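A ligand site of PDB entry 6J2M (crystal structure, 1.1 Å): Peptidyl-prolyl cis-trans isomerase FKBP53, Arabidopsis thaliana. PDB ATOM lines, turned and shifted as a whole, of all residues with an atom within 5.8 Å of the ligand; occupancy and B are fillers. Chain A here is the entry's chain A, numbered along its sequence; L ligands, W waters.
Water W2 lies within hydrogen-bond range of the side-chain carboxylate (OD2) of Asp 54 (2.7 Å) and an oxygen (O8) of the ligand (2.8 Å).
Water W3 lies within hydrogen-bond range of the side-chain hydroxyl of Ser 70 and an oxygen (O10) of the ligand.
An oxygen (O3) of the ligand lies within hydrogen-bond range of the side-chain hydroxyl (OH) of Tyr 98, at 2.7 Å.
O6 of the ligand sits at hydrogen-bond distance from OD2 of Asp 54, at 2.7 Å.
The backbone carbonyl oxygen (O) of Ser 70 is in hydrogen-bond range of an oxygen (O10) of the ligand (2.7 Å).
The backbone NH (N) of Ile 72 lies within hydrogen-bond range of an oxygen (O2) of the ligand (3.0 Å).
OH of Tyr 42 sits at hydrogen-bond distance from OD2 of Asp 54.
The backbone carbonyl oxygen (O) of Asp 54 lies within hydrogen-bond range of the backbone NH (N) of Gly 44 (2.8 Å).
O of Gly 44 lies within hydrogen-bond range of N of Phe 53.
CE2 of Tyr 42 touches O4 of the ligand, 3.4 Å away.
Phe 53 touches the ligand.
CZ of Phe 62 touches C40 of the ligand (3.5 Å).
CA of Val 71 touches O2 of the ligand (3.3 Å).
CE2 of Trp 75 touches C3 of the ligand, at 3.4 Å.
Gly 97 touches the ligand (O to C44, 3.3 Å).
Ile 107 touches the ligand (CD1 to C34, 3.4 Å).
Phe 115 touches the ligand.
12 residues have an atom within 4 Å of the ligand: Tyr 42, Phe 53, Asp 54, Phe 62, Ser 70, Val 71, Ile 72, Trp 75, Gly 97, Tyr 98, Ile 107 and Phe 115.
The nearest printed residue that does not touch the ligand is Gly 104 (4.2 Å).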
ATOM      1  N   TYR A  42      12.146  21.197 -14.017  1.00  0.00           N
ATOM      2  CA  TYR A  42      12.616  19.984 -14.692  1.00  0.00           C
ATOM      3  C   TYR A  42      13.976  19.502 -14.185  1.00  0.00           C
ATOM      4  O   TYR A  42      14.737  20.229 -13.565  1.00  0.00           O
ATOM      5  CB  TYR A  42      12.658  20.190 -16.212  1.00  0.00           C
ATOM      6  CG  TYR A  42      13.766  21.158 -16.647  1.00  0.00           C
ATOM      7  CD1 TYR A  42      13.552  22.563 -16.697  1.00  0.00           C
ATOM      8  CD2 TYR A  42      15.059  20.662 -16.965  1.00  0.00           C
ATOM      9  CE1 TYR A  42      14.596  23.432 -17.076  1.00  0.00           C
ATOM     10  CE2 TYR A  42      16.082  21.519 -17.341  1.00  0.00           C
ATOM     11  CZ  TYR A  42      15.855  22.903 -17.397  1.00  0.00           C
ATOM     12  OH  TYR A  42      16.849  23.798 -17.791  1.00  0.00           O
ATOM     13  N   GLY A  44      16.933  17.149 -16.394  1.00  0.00           N
ATOM     14  CA  GLY A  44      17.295  16.505 -17.658  1.00  0.00           C
ATOM     15  C   GLY A  44      18.446  15.541 -17.453  1.00  0.00           C
ATOM     16  O   GLY A  44      19.417  15.858 -16.761  1.00  0.00           O
ATOM     17  N   PHE A  53      22.262  16.255 -16.487  1.00  0.00           N
ATOM     18  CA  PHE A  53      22.956  17.402 -17.079  1.00  0.00           C
ATOM     19  C   PHE A  53      22.370  18.735 -16.663  1.00  0.00           C
ATOM     20  O   PHE A  53      23.065  19.733 -16.828  1.00  0.00           O
ATOM     21  CB  PHE A  53      23.049  17.305 -18.617  1.00  0.00           C
ATOM     22  CG  PHE A  53      21.772  17.094 -19.327  1.00  0.00           C
ATOM     23  CD1 PHE A  53      20.881  18.140 -19.539  1.00  0.00           C
ATOM     24  CD2 PHE A  53      21.402  15.843 -19.793  1.00  0.00           C
ATOM     25  CE1 PHE A  53      19.680  17.923 -20.200  1.00  0.00           C
ATOM     26  CE2 PHE A  53      20.222  15.645 -20.464  1.00  0.00           C
ATOM     27  CZ  PHE A  53      19.354  16.690 -20.635  1.00  0.00           C
ATOM     28  N   ASP A  54      21.139  18.817 -16.150  1.00  0.00           N
ATOM     29  CA  ASP A  54      20.586  20.125 -15.773  1.00  0.00           C
ATOM     30  C   ASP A  54      19.387  19.926 -14.892  1.00  0.00           C
ATOM     31  O   ASP A  54      18.663  18.919 -15.001  1.00  0.00           O
ATOM     32  CB  ASP A  54      20.232  20.941 -17.013  1.00  0.00           C
ATOM     33  CG  ASP A  54      20.012  22.408 -16.793  1.00  0.00           C
ATOM     34  OD1 ASP A  54      20.426  22.933 -15.724  1.00  0.00           O
ATOM     35  OD2 ASP A  54      19.402  23.047 -17.700  1.00  0.00           O
ATOM     36  N   PHE A  62      11.458  27.850 -15.585  1.00  0.00           N
ATOM     37  CA  PHE A  62      11.747  27.885 -17.009  1.00  0.00           C
ATOM     38  C   PHE A  62      10.448  28.088 -17.734  1.00  0.00           C
ATOM     39  O   PHE A  62       9.520  27.311 -17.589  1.00  0.00           O
ATOM     40  CB  PHE A  62      12.414  26.579 -17.455  1.00  0.00           C
ATOM     41  CG  PHE A  62      12.546  26.521 -18.941  1.00  0.00           C
ATOM     42  CD1 PHE A  62      13.413  27.359 -19.627  1.00  0.00           C
ATOM     43  CD2 PHE A  62      11.758  25.646 -19.677  1.00  0.00           C
ATOM     44  CE1 PHE A  62      13.443  27.370 -20.989  1.00  0.00           C
ATOM     45  CE2 PHE A  62      11.827  25.667 -21.071  1.00  0.00           C
ATOM     46  CZ  PHE A  62      12.658  26.509 -21.711  1.00  0.00           C
ATOM     47  N   SER A  70      10.425  26.315 -30.036  1.00  0.00           N
ATOM     48  CA  SER A  70      11.633  26.865 -29.427  1.00  0.00           C
ATOM     49  C   SER A  70      12.394  25.862 -28.569  1.00  0.00           C
ATOM     50  O   SER A  70      13.606  25.978 -28.385  1.00  0.00           O
ATOM     51  CB  SER A  70      11.343  28.141 -28.636  1.00  0.00           C
ATOM     52  OG  SER A  70      10.542  27.908 -27.484  1.00  0.00           O
ATOM     53  N   VAL A  71      11.674  24.909 -28.011  1.00  0.00           N
ATOM     54  CA  VAL A  71      12.237  23.781 -27.289  1.00  0.00           C
ATOM     55  C   VAL A  71      12.348  22.583 -28.224  1.00  0.00           C
ATOM     56  O   VAL A  71      11.707  22.548 -29.301  1.00  0.00           O
ATOM     57  CB  VAL A  71      11.405  23.439 -26.047  1.00  0.00           C
ATOM     58  CG1 VAL A  71      11.496  24.498 -24.997  1.00  0.00           C
ATOM     59  CG2 VAL A  71       9.963  23.107 -26.398  1.00  0.00           C
ATOM     60  N   ILE A  72      13.085  21.583 -27.798  1.00  0.00           N
ATOM     61  CA  ILE A  72      13.112  20.305 -28.490  1.00  0.00           C
ATOM     62  C   ILE A  72      11.707  19.732 -28.644  1.00  0.00           C
ATOM     63  O   ILE A  72      10.816  19.950 -27.805  1.00  0.00           O
ATOM     64  CB  ILE A  72      14.079  19.309 -27.796  1.00  0.00           C
ATOM     65  CG1 ILE A  72      13.683  19.050 -26.324  1.00  0.00           C
ATOM     66  CG2 ILE A  72      15.516  19.810 -27.936  1.00  0.00           C
ATOM     67  CD1 ILE A  72      14.537  17.979 -25.675  1.00  0.00           C
ATOM     68  N   TRP A  75       9.729  18.045 -25.837  1.00  0.00           N
ATOM     69  CA  TRP A  75       9.045  18.928 -24.882  1.00  0.00           C
ATOM     70  C   TRP A  75       7.748  19.523 -25.460  1.00  0.00           C
ATOM     71  O   TRP A  75       6.760  19.579 -24.724  1.00  0.00           O
ATOM     72  CB  TRP A  75       9.974  20.047 -24.454  1.00  0.00           C
ATOM     73  CG  TRP A  75      10.818  19.739 -23.254  1.00  0.00           C
ATOM     74  CD1 TRP A  75      11.709  18.727 -23.078  1.00  0.00           C
ATOM     75  CD2 TRP A  75      10.826  20.496 -22.036  1.00  0.00           C
ATOM     76  NE1 TRP A  75      12.249  18.782 -21.827  1.00  0.00           N
ATOM     77  CE2 TRP A  75      11.735  19.870 -21.175  1.00  0.00           C
ATOM     78  CE3 TRP A  75      10.139  21.619 -21.615  1.00  0.00           C
ATOM     79  CZ2 TRP A  75      11.996  20.371 -19.905  1.00  0.00           C
ATOM     80  CZ3 TRP A  75      10.399  22.126 -20.366  1.00  0.00           C
ATOM     81  CH2 TRP A  75      11.319  21.527 -19.520  1.00  0.00           C
ATOM     82  N   GLY A  97      15.016  15.288 -29.825  1.00  0.00           N
ATOM     83  CA  GLY A  97      15.936  16.046 -28.967  1.00  0.00           C
ATOM     84  C   GLY A  97      16.849  16.855 -29.864  1.00  0.00           C
ATOM     85  O   GLY A  97      16.384  17.632 -30.681  1.00  0.00           O
ATOM     86  N   TYR A  98      18.140  16.637 -29.686  1.00  0.00           N
ATOM     87  CA  TYR A  98      19.151  17.432 -30.402  1.00  0.00           C
ATOM     88  C   TYR A  98      19.755  16.710 -31.591  1.00  0.00           C
ATOM     89  O   TYR A  98      20.604  17.244 -32.267  1.00  0.00           O
ATOM     90  CB  TYR A  98      20.237  17.914 -29.438  1.00  0.00           C
ATOM     91  CG  TYR A  98      19.675  18.787 -28.368  1.00  0.00           C
ATOM     92  CD1 TYR A  98      19.423  20.127 -28.634  1.00  0.00           C
ATOM     93  CD2 TYR A  98      19.380  18.331 -27.104  1.00  0.00           C
ATOM     94  CE1 TYR A  98      18.866  20.949 -27.656  1.00  0.00           C
ATOM     95  CE2 TYR A  98      18.831  19.129 -26.134  1.00  0.00           C
ATOM     96  CZ  TYR A  98      18.600  20.461 -26.381  1.00  0.00           C
ATOM     97  OH  TYR A  98      18.060  21.301 -25.454  1.00  0.00           O
ATOM     98  N   GLY A  99      19.275  15.486 -31.875  1.00  0.00           N
ATOM     99  CA  GLY A  99      19.720  14.814 -33.083  1.00  0.00           C
ATOM    100  C   GLY A  99      21.222  14.587 -33.098  1.00  0.00           C
ATOM    101  O   GLY A  99      21.803  14.244 -32.055  1.00  0.00           O
ATOM    102  N   ALA A 103      24.258  19.200 -27.523  1.00  0.00           N
ATOM    103  CA  ALA A 103      23.969  20.488 -26.832  1.00  0.00           C
ATOM    104  C   ALA A 103      24.779  20.830 -25.583  1.00  0.00           C
ATOM    105  O   ALA A 103      25.024  19.982 -24.778  1.00  0.00           O
ATOM    106  CB  ALA A 103      22.505  20.555 -26.401  1.00  0.00           C
ATOM    107  N   GLY A 104      24.951  22.132 -25.317  1.00  0.00           N
ATOM    108  CA  GLY A 104      25.502  22.584 -24.041  1.00  0.00           C
ATOM    109  C   GLY A 104      26.883  22.055 -23.679  1.00  0.00           C
ATOM    110  O   GLY A 104      27.325  22.379 -22.554  1.00  0.00           O
ATOM    111  N   GLN A 106      27.180  19.181 -23.038  1.00  0.00           N
ATOM    112  CA  GLN A 106      26.662  18.301 -22.061  1.00  0.00           C
ATOM    113  C   GLN A 106      25.925  17.070 -22.573  1.00  0.00           C
ATOM    114  O   GLN A 106      25.855  16.043 -21.912  1.00  0.00           O
ATOM    115  CB  GLN A 106      25.695  19.095 -21.217  1.00  0.00           C
ATOM    116  N   ILE A 107      25.378  17.194 -23.760  1.00  0.00           N
ATOM    117  CA  ILE A 107      24.580  16.145 -24.345  1.00  0.00           C
ATOM    118  C   ILE A 107      25.414  15.769 -25.590  1.00  0.00           C
ATOM    119  O   ILE A 107      25.567  16.571 -26.500  1.00  0.00           O
ATOM    120  CB  ILE A 107      23.177  16.648 -24.706  1.00  0.00           C
ATOM    121  CG1 ILE A 107      22.400  16.998 -23.375  1.00  0.00           C
ATOM    122  CG2 ILE A 107      22.444  15.588 -25.525  1.00  0.00           C
ATOM    123  CD1 ILE A 107      21.020  17.599 -23.695  1.00  0.00           C
ATOM    124  N   LEU A 113      17.122  11.128 -24.418  1.00  0.00           N
ATOM    125  CA  LEU A 113      17.045  11.985 -23.242  1.00  0.00           C
ATOM    126  C   LEU A 113      15.882  11.541 -22.364  1.00  0.00           C
ATOM    127  O   LEU A 113      14.855  11.061 -22.864  1.00  0.00           O
ATOM    128  CB  LEU A 113      16.830  13.441 -23.634  1.00  0.00           C
ATOM    129  CG  LEU A 113      17.825  14.007 -24.588  1.00  0.00           C
ATOM    130  CD1 LEU A 113      17.444  15.435 -25.005  1.00  0.00           C
ATOM    131  CD2 LEU A 113      19.229  13.998 -23.997  1.00  0.00           C
ATOM    132  N   PHE A 115      13.542  13.452 -19.264  1.00  0.00           N
ATOM    133  CA  PHE A 115      13.277  14.606 -18.411  1.00  0.00           C
ATOM    134  C   PHE A 115      12.153  14.265 -17.445  1.00  0.00           C
ATOM    135  O   PHE A 115      11.140  13.708 -17.839  1.00  0.00           O
ATOM    136  CB  PHE A 115      12.855  15.869 -19.157  1.00  0.00           C
ATOM    137  CG  PHE A 115      13.927  16.530 -19.949  1.00  0.00           C
ATOM    138  CD1 PHE A 115      14.305  16.069 -21.216  1.00  0.00           C
ATOM    139  CD2 PHE A 115      14.551  17.679 -19.474  1.00  0.00           C
ATOM    140  CE1 PHE A 115      15.248  16.721 -21.973  1.00  0.00           C
ATOM    141  CE2 PHE A 115      15.495  18.338 -20.225  1.00  0.00           C
ATOM    142  CZ  PHE A 115      15.844  17.880 -21.489  1.00  0.00           C
HETATM  143  C1  LIG L   1      15.474  22.795 -24.608  1.00  0.00           C
HETATM  144  C2  LIG L   1      15.522  21.814 -23.441  1.00  0.00           C
HETATM  145  C3  LIG L   1      14.119  21.622 -22.873  1.00  0.00           C
HETATM  146  C4  LIG L   1      13.704  22.818 -22.047  1.00  0.00           C
HETATM  147  C5  LIG L   1      14.681  23.028 -20.914  1.00  0.00           C
HETATM  148  C6  LIG L   1      16.097  23.227 -21.463  1.00  0.00           C
HETATM  149  C7  LIG L   1      17.569  21.365 -22.196  1.00  0.00           C
HETATM  150  C8  LIG L   1      18.468  21.576 -21.034  1.00  0.00           C
HETATM  151  C9  LIG L   1      19.730  22.434 -21.243  1.00  0.00           C
HETATM  152  C10 LIG L   1      20.559  22.059 -22.444  1.00  0.00           C
HETATM  153  C11 LIG L   1      21.522  23.171 -22.752  1.00  0.00           C
HETATM  154  C12 LIG L   1      20.845  24.504 -22.909  1.00  0.00           C
HETATM  155  C13 LIG L   1      20.024  24.835 -21.694  1.00  0.00           C
HETATM  156  C14 LIG L   1      19.032  25.992 -21.810  1.00  0.00           C
HETATM  157  C15 LIG L   1      19.488  27.281 -22.499  1.00  0.00           C
HETATM  158  C16 LIG L   1      20.202  28.328 -21.649  1.00  0.00           C
HETATM  159  C17 LIG L   1      20.631  29.473 -22.562  1.00  0.00           C
HETATM  160  C18 LIG L   1      19.554  30.051 -23.440  1.00  0.00           C
HETATM  161  C19 LIG L   1      19.657  29.928 -24.751  1.00  0.00           C
HETATM  162  C20 LIG L   1      18.688  30.343 -25.804  1.00  0.00           C
HETATM  163  C21 LIG L   1      18.020  29.077 -26.295  1.00  0.00           C
HETATM  164  C22 LIG L   1      16.750  28.673 -25.710  1.00  0.00           C
HETATM  165  C23 LIG L   1      16.233  27.302 -26.110  1.00  0.00           C
HETATM  166  C24 LIG L   1      16.391  26.254 -24.997  1.00  0.00           C
HETATM  167  C25 LIG L   1      16.172  24.844 -25.605  1.00  0.00           C
HETATM  168  C26 LIG L   1      17.148  24.507 -26.686  1.00  0.00           C
HETATM  169  C27 LIG L   1      16.658  24.327 -27.921  1.00  0.00           C
HETATM  170  C28 LIG L   1      17.429  24.198 -29.217  1.00  0.00           C
HETATM  171  C29 LIG L   1      16.778  23.102 -30.087  1.00  0.00           C
HETATM  172  C30 LIG L   1      17.456  22.995 -31.431  1.00  0.00           C
HETATM  173  C31 LIG L   1      17.434  24.314 -32.169  1.00  0.00           C
HETATM  174  C32 LIG L   1      18.090  25.388 -31.320  1.00  0.00           C
HETATM  175  C33 LIG L   1      17.417  25.516 -29.956  1.00  0.00           C
HETATM  176  C34 LIG L   1      21.286  20.729 -22.285  1.00  0.00           C
HETATM  177  C35 LIG L   1      21.422  27.820 -20.914  1.00  0.00           C
HETATM  178  C36 LIG L   1      18.396  30.697 -22.739  1.00  0.00           C
HETATM  179  C37 LIG L   1      19.380  31.098 -26.934  1.00  0.00           C
HETATM  180  C38 LIG L   1      18.364  31.724 -27.947  1.00  0.00           C
HETATM  181  C39 LIG L   1      18.298  31.392 -29.140  1.00  0.00           C
HETATM  182  C40 LIG L   1      15.436  26.518 -23.845  1.00  0.00           C
HETATM  183  C41 LIG L   1      18.590  24.505 -26.312  1.00  0.00           C
HETATM  184  C42 LIG L   1      22.225  25.656 -24.483  1.00  0.00           C
HETATM  185  C43 LIG L   1      17.235  26.774 -20.396  1.00  0.00           C
HETATM  186  C44 LIG L   1      16.900  20.696 -31.927  1.00  0.00           C
HETATM  187  N1  LIG L   1      16.473  22.126 -22.363  1.00  0.00           N
HETATM  188  O1  LIG L   1      16.255  23.873 -24.498  1.00  0.00           O
HETATM  189  O2  LIG L   1      14.743  22.614 -25.533  1.00  0.00           O
HETATM  190  O3  LIG L   1      17.867  20.430 -22.933  1.00  0.00           O
HETATM  191  O4  LIG L   1      18.216  21.048 -19.966  1.00  0.00           O
HETATM  192  O5  LIG L   1      19.129  23.723 -21.415  1.00  0.00           O
HETATM  193  O6  LIG L   1      20.517  22.407 -20.074  1.00  0.00           O
HETATM  194  O7  LIG L   1      21.814  25.539 -23.096  1.00  0.00           O
HETATM  195  O8  LIG L   1      18.558  26.208 -20.460  1.00  0.00           O
HETATM  196  O9  LIG L   1      18.577  28.365 -27.081  1.00  0.00           O
HETATM  197  O10 LIG L   1      14.846  27.448 -26.470  1.00  0.00           O
HETATM  198  O11 LIG L   1      16.779  22.044 -32.299  1.00  0.00           O
HETATM  199  O12 LIG L   1      18.077  24.176 -33.430  1.00  0.00           O
HETATM  200  O   HOH W   1      18.882  21.808 -34.666  1.00  0.00           O
HETATM  201  O   HOH W   2      19.890  25.715 -18.088  1.00  0.00           O
HETATM  202  O   HOH W   3      12.272  27.778 -25.404  1.00  0.00           O
